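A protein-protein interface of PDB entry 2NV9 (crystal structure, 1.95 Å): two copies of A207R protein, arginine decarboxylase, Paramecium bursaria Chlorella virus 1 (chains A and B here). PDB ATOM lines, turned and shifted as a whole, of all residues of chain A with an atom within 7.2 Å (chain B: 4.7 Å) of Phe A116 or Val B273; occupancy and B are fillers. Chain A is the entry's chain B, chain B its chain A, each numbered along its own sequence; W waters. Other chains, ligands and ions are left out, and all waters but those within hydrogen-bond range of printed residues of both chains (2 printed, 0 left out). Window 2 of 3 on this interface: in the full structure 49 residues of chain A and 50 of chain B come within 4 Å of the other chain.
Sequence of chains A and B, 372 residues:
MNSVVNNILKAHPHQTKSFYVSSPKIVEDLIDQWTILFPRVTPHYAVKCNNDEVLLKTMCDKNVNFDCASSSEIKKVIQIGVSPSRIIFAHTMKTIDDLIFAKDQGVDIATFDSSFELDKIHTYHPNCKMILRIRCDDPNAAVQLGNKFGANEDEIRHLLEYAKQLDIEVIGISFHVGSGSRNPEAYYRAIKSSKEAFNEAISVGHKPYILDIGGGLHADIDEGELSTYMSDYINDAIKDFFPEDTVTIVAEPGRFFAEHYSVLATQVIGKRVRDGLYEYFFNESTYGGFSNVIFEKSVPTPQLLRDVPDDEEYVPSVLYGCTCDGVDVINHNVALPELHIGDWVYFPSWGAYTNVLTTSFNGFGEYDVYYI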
ATOM      1  N   MET A  93      -6.430   6.161   5.291  1.00  0.00           N
ATOM      2  CA  MET A  93      -6.270   5.666   3.928  1.00  0.00           C
ATOM      3  C   MET A  93      -6.973   6.576   2.926  1.00  0.00           C
ATOM      4  O   MET A  93      -8.201   6.589   2.839  1.00  0.00           O
ATOM      5  CB  MET A  93      -6.808   4.238   3.810  1.00  0.00           C
ATOM      6  CG  MET A  93      -5.973   3.199   4.539  1.00  0.00           C
ATOM      7  SD  MET A  93      -4.300   3.063   3.882  1.00  0.00           S
ATOM      8  CE  MET A  93      -3.550   1.969   5.084  1.00  0.00           C
ATOM      9  N   ASP A 113      -1.536   5.675   9.423  1.00  0.00           N
ATOM     10  CA  ASP A 113      -1.171   4.516  10.264  1.00  0.00           C
ATOM     11  C   ASP A 113      -0.245   3.523   9.544  1.00  0.00           C
ATOM     12  O   ASP A 113      -0.062   2.388  10.022  1.00  0.00           O
ATOM     13  CB  ASP A 113      -2.432   3.859  10.858  1.00  0.00           C
ATOM     14  CG  ASP A 113      -3.392   3.263   9.786  1.00  0.00           C
ATOM     15  OD1 ASP A 113      -2.938   2.875   8.680  1.00  0.00           O
ATOM     16  OD2 ASP A 113      -4.602   3.151  10.095  1.00  0.00           O
ATOM     17  N   SER A 114       0.361   3.973   8.425  1.00  0.00           N
ATOM     18  CA  SER A 114       1.202   3.096   7.579  1.00  0.00           C
ATOM     19  C   SER A 114       2.307   3.859   6.893  1.00  0.00           C
ATOM     20  O   SER A 114       2.149   5.056   6.601  1.00  0.00           O
ATOM     21  CB  SER A 114       0.371   2.357   6.508  1.00  0.00           C
ATOM     22  OG  SER A 114      -0.177   3.272   5.563  1.00  0.00           O
ATOM     23  N   SER A 115       3.399   3.168   6.596  1.00  0.00           N
ATOM     24  CA  SER A 115       4.533   3.790   5.903  1.00  0.00           C
ATOM     25  C   SER A 115       4.187   4.136   4.449  1.00  0.00           C
ATOM     26  O   SER A 115       4.601   5.190   3.941  1.00  0.00           O
ATOM     27  CB  SER A 115       5.776   2.900   5.953  1.00  0.00           C
ATOM     28  OG  SER A 115       5.530   1.668   5.287  1.00  0.00           O
ATOM     29  N   PHE A 116       3.425   3.259   3.794  1.00  0.00           N
ATOM     30  CA  PHE A 116       2.951   3.558   2.429  1.00  0.00           C
ATOM     31  C   PHE A 116       2.073   4.819   2.359  1.00  0.00           C
ATOM     32  O   PHE A 116       2.059   5.526   1.321  1.00  0.00           O
ATOM     33  CB  PHE A 116       2.243   2.369   1.778  1.00  0.00           C
ATOM     34  CG  PHE A 116       3.145   1.192   1.519  1.00  0.00           C
ATOM     35  CD1 PHE A 116       3.965   1.168   0.408  1.00  0.00           C
ATOM     36  CD2 PHE A 116       3.180   0.111   2.396  1.00  0.00           C
ATOM     37  CE1 PHE A 116       4.815   0.122   0.173  1.00  0.00           C
ATOM     38  CE2 PHE A 116       4.036  -0.970   2.169  1.00  0.00           C
ATOM     39  CZ  PHE A 116       4.838  -0.978   1.058  1.00  0.00           C
ATOM     40  N   GLU A 117       1.354   5.110   3.440  1.00  0.00           N
ATOM     41  CA  GLU A 117       0.590   6.347   3.499  1.00  0.00           C
ATOM     42  C   GLU A 117       1.491   7.589   3.481  1.00  0.00           C
ATOM     43  O   GLU A 117       1.140   8.614   2.855  1.00  0.00           O
ATOM     44  CB  GLU A 117      -0.379   6.393   4.692  1.00  0.00           C
ATOM     45  CG  GLU A 117      -1.561   7.424   4.489  1.00  0.00           C
ATOM     46  CD  GLU A 117      -2.607   7.030   3.401  1.00  0.00           C
ATOM     47  OE1 GLU A 117      -2.554   5.899   2.853  1.00  0.00           O
ATOM     48  OE2 GLU A 117      -3.541   7.820   3.153  1.00  0.00           O
ATOM     49  N   LEU A 118       2.630   7.488   4.186  1.00  0.00           N
ATOM     50  CA  LEU A 118       3.651   8.531   4.183  1.00  0.00           C
ATOM     51  C   LEU A 118       4.334   8.716   2.839  1.00  0.00           C
ATOM     52  O   LEU A 118       4.679   9.841   2.505  1.00  0.00           O
ATOM     53  CB  LEU A 118       4.723   8.337   5.283  1.00  0.00           C
ATOM     54  CG  LEU A 118       4.243   8.287   6.745  1.00  0.00           C
ATOM     55  CD1 LEU A 118       5.319   7.786   7.724  1.00  0.00           C
ATOM     56  CD2 LEU A 118       3.748   9.676   7.161  1.00  0.00           C
ATOM     57  N   ASP A 119       4.558   7.622   2.106  1.00  0.00           N
ATOM     58  CA  ASP A 119       5.038   7.660   0.717  1.00  0.00           C
ATOM     59  C   ASP A 119       4.142   8.505  -0.204  1.00  0.00           C
ATOM     60  O   ASP A 119       4.651   9.334  -0.983  1.00  0.00           O
ATOM     61  CB  ASP A 119       5.211   6.268   0.115  1.00  0.00           C
ATOM     62  CG  ASP A 119       6.253   5.444   0.846  1.00  0.00           C
ATOM     63  OD1 ASP A 119       7.128   6.038   1.497  1.00  0.00           O
ATOM     64  OD2 ASP A 119       6.187   4.210   0.745  1.00  0.00           O
ATOM     65  N   LYS A 120       2.833   8.300  -0.079  1.00  0.00           N
ATOM     66  CA  LYS A 120       1.818   9.090  -0.791  1.00  0.00           C
ATOM     67  C   LYS A 120       1.832  10.575  -0.377  1.00  0.00           C
ATOM     68  O   LYS A 120       1.754  11.456  -1.230  1.00  0.00           O
ATOM     69  CB  LYS A 120       0.420   8.480  -0.570  1.00  0.00           C
ATOM     70  CG  LYS A 120       0.105   7.301  -1.478  1.00  0.00           C
ATOM     71  CD  LYS A 120      -0.823   6.284  -0.775  1.00  0.00           C
ATOM     72  CE  LYS A 120      -2.231   6.747  -0.686  1.00  0.00           C
ATOM     73  NZ  LYS A 120      -3.117   5.946   0.232  1.00  0.00           N
ATOM     74  N   ILE A 121       1.924  10.835   0.927  1.00  0.00           N
ATOM     75  CA  ILE A 121       1.995  12.211   1.427  1.00  0.00           C
ATOM     76  C   ILE A 121       3.227  12.912   0.846  1.00  0.00           C
ATOM     77  O   ILE A 121       3.127  14.013   0.315  1.00  0.00           O
ATOM     78  CB  ILE A 121       2.033  12.295   2.980  1.00  0.00           C
ATOM     79  CG1 ILE A 121       0.687  11.895   3.611  1.00  0.00           C
ATOM     80  CG2 ILE A 121       2.485  13.740   3.444  1.00  0.00           C
ATOM     81  CD1 ILE A 121      -0.552  12.675   3.099  1.00  0.00           C
ATOM     82  N   HIS A 122       4.380  12.251   0.939  1.00  0.00           N
ATOM     83  CA  HIS A 122       5.630  12.790   0.411  1.00  0.00           C
ATOM     84  C   HIS A 122       5.511  13.156  -1.056  1.00  0.00           C
ATOM     85  O   HIS A 122       5.973  14.234  -1.475  1.00  0.00           O
ATOM     86  CB  HIS A 122       6.820  11.806   0.646  1.00  0.00           C
ATOM     87  CG  HIS A 122       8.134  12.290   0.090  1.00  0.00           C
ATOM     88  ND1 HIS A 122       9.008  13.068   0.819  1.00  0.00           N
ATOM     89  CD2 HIS A 122       8.716  12.107  -1.122  1.00  0.00           C
ATOM     90  CE1 HIS A 122      10.073  13.343   0.083  1.00  0.00           C
ATOM     91  NE2 HIS A 122       9.916  12.781  -1.106  1.00  0.00           N
ATOM     92  N   GLU A 155       5.009  -0.607  16.281  1.00  0.00           N
ATOM     93  CA  GLU A 155       5.363   0.118  15.061  1.00  0.00           C
ATOM     94  C   GLU A 155       5.337   1.652  15.180  1.00  0.00           C
ATOM     95  O   GLU A 155       5.701   2.357  14.244  1.00  0.00           O
ATOM     96  CB  GLU A 155       4.509  -0.402  13.892  1.00  0.00           C
ATOM     97  CG  GLU A 155       3.034   0.002  13.940  1.00  0.00           C
ATOM     98  CD  GLU A 155       2.132  -0.744  12.926  1.00  0.00           C
ATOM     99  OE1 GLU A 155       2.581  -1.165  11.836  1.00  0.00           O
ATOM    100  OE2 GLU A 155       0.932  -0.879  13.202  1.00  0.00           O
ATOM    101  N   LEU A 159       7.173   4.235  12.453  1.00  0.00           N
ATOM    102  CA  LEU A 159       6.344   5.167  11.661  1.00  0.00           C
ATOM    103  C   LEU A 159       6.758   6.622  11.867  1.00  0.00           C
ATOM    104  O   LEU A 159       6.808   7.410  10.903  1.00  0.00           O
ATOM    105  CB  LEU A 159       4.857   4.958  11.937  1.00  0.00           C
ATOM    106  CG  LEU A 159       4.259   3.622  11.463  1.00  0.00           C
ATOM    107  CD1 LEU A 159       2.847   3.425  12.036  1.00  0.00           C
ATOM    108  CD2 LEU A 159       4.237   3.551   9.943  1.00  0.00           C
ATOM    109  N   TYR A 162      10.108   7.231  10.182  1.00  0.00           N
ATOM    110  CA  TYR A 162       9.918   7.207   8.730  1.00  0.00           C
ATOM    111  C   TYR A 162       9.405   8.547   8.220  1.00  0.00           C
ATOM    112  O   TYR A 162       9.879   9.038   7.187  1.00  0.00           O
ATOM    113  CB  TYR A 162       8.970   6.089   8.324  1.00  0.00           C
ATOM    114  CG  TYR A 162       8.997   5.784   6.851  1.00  0.00           C
ATOM    115  CD1 TYR A 162      10.184   5.404   6.228  1.00  0.00           C
ATOM    116  CD2 TYR A 162       7.858   5.942   6.052  1.00  0.00           C
ATOM    117  CE1 TYR A 162      10.219   5.134   4.893  1.00  0.00           C
ATOM    118  CE2 TYR A 162       7.879   5.670   4.694  1.00  0.00           C
ATOM    119  CZ  TYR A 162       9.052   5.261   4.128  1.00  0.00           C
ATOM    120  OH  TYR A 162       9.140   4.991   2.786  1.00  0.00           O
ATOM    121  N   LYS B 271      -2.020   0.588   1.352  1.00  0.00           N
ATOM    122  CA  LYS B 271      -1.243  -0.621   1.639  1.00  0.00           C
ATOM    123  C   LYS B 271      -0.593  -0.532   3.013  1.00  0.00           C
ATOM    124  O   LYS B 271      -0.163   0.532   3.457  1.00  0.00           O
ATOM    125  CB  LYS B 271      -0.151  -0.845   0.580  1.00  0.00           C
ATOM    126  CG  LYS B 271       0.535  -2.217   0.634  1.00  0.00           C
ATOM    127  CD  LYS B 271       1.568  -2.329  -0.464  1.00  0.00           C
ATOM    128  CE  LYS B 271       2.356  -3.627  -0.402  1.00  0.00           C
ATOM    129  NZ  LYS B 271       3.273  -3.788  -1.598  1.00  0.00           N
ATOM    130  N   ARG B 272      -0.581  -1.665   3.705  1.00  0.00           N
ATOM    131  CA  ARG B 272       0.082  -1.743   4.979  1.00  0.00           C
ATOM    132  C   ARG B 272       0.587  -3.173   5.126  1.00  0.00           C
ATOM    133  O   ARG B 272      -0.165  -4.125   4.891  1.00  0.00           O
ATOM    134  CB  ARG B 272      -0.912  -1.279   6.067  1.00  0.00           C
ATOM    135  CG  ARG B 272      -0.372  -1.198   7.498  1.00  0.00           C
ATOM    136  CD  ARG B 272      -1.416  -0.656   8.481  1.00  0.00           C
ATOM    137  NE  ARG B 272      -2.618  -1.507   8.489  1.00  0.00           N
ATOM    138  CZ  ARG B 272      -3.882  -1.050   8.461  1.00  0.00           C
ATOM    139  NH1 ARG B 272      -4.141   0.256   8.521  1.00  0.00           N
ATOM    140  NH2 ARG B 272      -4.879  -1.912   8.454  1.00  0.00           N
ATOM    141  N   VAL B 273       1.878  -3.325   5.451  1.00  0.00           N
ATOM    142  CA  VAL B 273       2.464  -4.652   5.594  1.00  0.00           C
ATOM    143  C   VAL B 273       2.970  -4.783   7.023  1.00  0.00           C
ATOM    144  O   VAL B 273       3.787  -3.968   7.485  1.00  0.00           O
ATOM    145  CB  VAL B 273       3.613  -4.900   4.604  1.00  0.00           C
ATOM    146  CG1 VAL B 273       4.197  -6.331   4.780  1.00  0.00           C
ATOM    147  CG2 VAL B 273       3.158  -4.669   3.171  1.00  0.00           C
ATOM    148  N   ARG B 274       2.454  -5.785   7.728  1.00  0.00           N
ATOM    149  CA  ARG B 274       2.826  -5.985   9.141  1.00  0.00           C
ATOM    150  C   ARG B 274       3.056  -7.456   9.460  1.00  0.00           C
ATOM    151  O   ARG B 274       2.157  -8.272   9.313  1.00  0.00           O
ATOM    152  CB  ARG B 274       1.762  -5.402  10.080  1.00  0.00           C
ATOM    153  CG  ARG B 274       1.338  -3.963   9.756  1.00  0.00           C
ATOM    154  CD  ARG B 274       0.598  -3.317  10.909  1.00  0.00           C
ATOM    155  NE  ARG B 274      -0.813  -3.603  10.853  1.00  0.00           N
ATOM    156  CZ  ARG B 274      -1.748  -2.862  11.431  1.00  0.00           C
ATOM    157  NH1 ARG B 274      -1.409  -1.773  12.128  1.00  0.00           N
ATOM    158  NH2 ARG B 274      -3.023  -3.220  11.312  1.00  0.00           N
ATOM    159  N   ASP B 275       4.281  -7.764   9.882  1.00  0.00           N
ATOM    160  CA  ASP B 275       4.703  -9.108  10.287  1.00  0.00           C
ATOM    161  C   ASP B 275       4.279 -10.197   9.296  1.00  0.00           C
ATOM    162  O   ASP B 275       3.706 -11.225   9.686  1.00  0.00           O
ATOM    163  CB  ASP B 275       4.182  -9.436  11.690  1.00  0.00           C
ATOM    164  CG  ASP B 275       4.756  -8.528  12.769  1.00  0.00           C
ATOM    165  OD1 ASP B 275       5.976  -8.293  12.793  1.00  0.00           O
ATOM    166  OD2 ASP B 275       3.957  -8.054  13.594  1.00  0.00           O
ATOM    167  N   LEU B 277       1.974 -10.086   6.963  1.00  0.00           N
ATOM    168  CA  LEU B 277       0.587  -9.961   6.462  1.00  0.00           C
ATOM    169  C   LEU B 277       0.387  -8.707   5.584  1.00  0.00           C
ATOM    170  O   LEU B 277       0.699  -7.598   6.011  1.00  0.00           O
ATOM    171  CB  LEU B 277      -0.398  -9.949   7.635  1.00  0.00           C
ATOM    172  CG  LEU B 277      -1.908 -10.008   7.340  1.00  0.00           C
ATOM    173  CD1 LEU B 277      -2.314 -11.334   6.613  1.00  0.00           C
ATOM    174  CD2 LEU B 277      -2.689  -9.832   8.671  1.00  0.00           C
ATOM    175  N   TYR B 278      -0.151  -8.892   4.382  1.00  0.00           N
ATOM    176  CA  TYR B 278      -0.256  -7.795   3.378  1.00  0.00           C
ATOM    177  C   TYR B 278      -1.665  -7.213   3.361  1.00  0.00           C
ATOM    178  O   TYR B 278      -2.585  -7.860   2.889  1.00  0.00           O
ATOM    179  CB  TYR B 278       0.182  -8.285   1.995  1.00  0.00           C
ATOM    180  CG  TYR B 278       1.659  -8.616   1.959  1.00  0.00           C
ATOM    181  CD1 TYR B 278       2.573  -7.794   1.265  1.00  0.00           C
ATOM    182  CD2 TYR B 278       2.157  -9.732   2.641  1.00  0.00           C
ATOM    183  CE1 TYR B 278       3.937  -8.080   1.242  1.00  0.00           C
ATOM    184  CE2 TYR B 278       3.532 -10.027   2.646  1.00  0.00           C
ATOM    185  CZ  TYR B 278       4.413  -9.202   1.941  1.00  0.00           C
ATOM    186  OH  TYR B 278       5.747  -9.497   1.928  1.00  0.00           O
ATOM    187  N   ILE B 341       0.119  -0.111  -4.543  1.00  0.00           N
ATOM    188  CA  ILE B 341      -0.769   1.017  -4.706  1.00  0.00           C
ATOM    189  C   ILE B 341      -0.770   1.414  -6.212  1.00  0.00           C
ATOM    190  O   ILE B 341       0.288   1.616  -6.811  1.00  0.00           O
ATOM    191  CB  ILE B 341      -0.394   2.215  -3.799  1.00  0.00           C
ATOM    192  CG1 ILE B 341      -0.722   1.915  -2.337  1.00  0.00           C
ATOM    193  CG2 ILE B 341      -1.169   3.506  -4.277  1.00  0.00           C
ATOM    194  CD1 ILE B 341      -0.073   2.918  -1.337  1.00  0.00           C
HETATM  195  O   HOH W   1      -1.158   3.387   2.264  1.00  0.00           O
HETATM  196  O   HOH W   2       3.438  -0.939   5.783  1.00  0.00           O
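Water W2 lies within hydrogen-bond range of the backbone NH (N) of Val B273 (2.9 Å) and the side-chain hydroxyl (OG) of Ser A115 (3.4 Å). Water W1 lies within hydrogen-bond range of OE1 of Glu A117 (2.9 Å), N of Lys B271 (3.1 Å), OG of Ser A114 (3.4 Å) and SD of Met A93 (3.5 Å).
Of the printed residues of chain B, Met A93 touches Arg B272 (3.9 Å). Printed residues of chain B within 4 Å of Asp A113: Arg B272. His A122 touches none of the printed residues of chain B. Printed residues of chain B within 4 Å of Glu A155: Arg B274. Val B273 touches one residue of chain A. The nearest residue of chain B that does not touch Phe A116 is Arg B272 (4.4 Å). The nearest residue of chain A that does not touch Val B273 is Glu A155 (5.3 Å). The nearest printed residue of chain A that does not touch Ile B341 is Glu A117 (5.4 Å).
Among the printed residues, pairs that only touch across the chains: Phe A116 with Lys B271 (3.5 Å), Lys A120 with Ile B341 (3.5 Å), Ser A114 with Arg B272 (3.8 Å), Met A93 with Arg B272 (3.9 Å), Phe A116 with Ile B341 (3.9 Å) and Phe A116 with Val B273 (3.9 Å).
OG of Ser A114 is in hydrogen-bond range of N of Glu A117 (3.2 Å). The side-chain carboxylate of Glu A117 lies within salt-bridge range of the side-chain amino group of Lys A120 (2.7 Å).
No position is printed for both chains. Of the 9 pairs that touch across the chains among the printed residues, none has its exchanged pair printed and touching as well.
Hydrophobic or aromatic side chains of chain B that line the printed part of chain A: Val B273 and Ile B341. Of the 14 printed residues of chain A, 6 touch a printed residue of chain B. Among the printed residues, 9 pairs touch across the chains.
The backbone carbonyl oxygen (O) of Lys B271 sits at hydrogen-bond distance from the side-chain hydroxyl (OG) of Ser A114. OE2 of Glu A155 is in salt-bridge range of NH1 of Arg B274 (2.7 Å). NH1 of Arg B272 is in salt-bridge range of OD1 of Asp A113 (2.9 Å).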
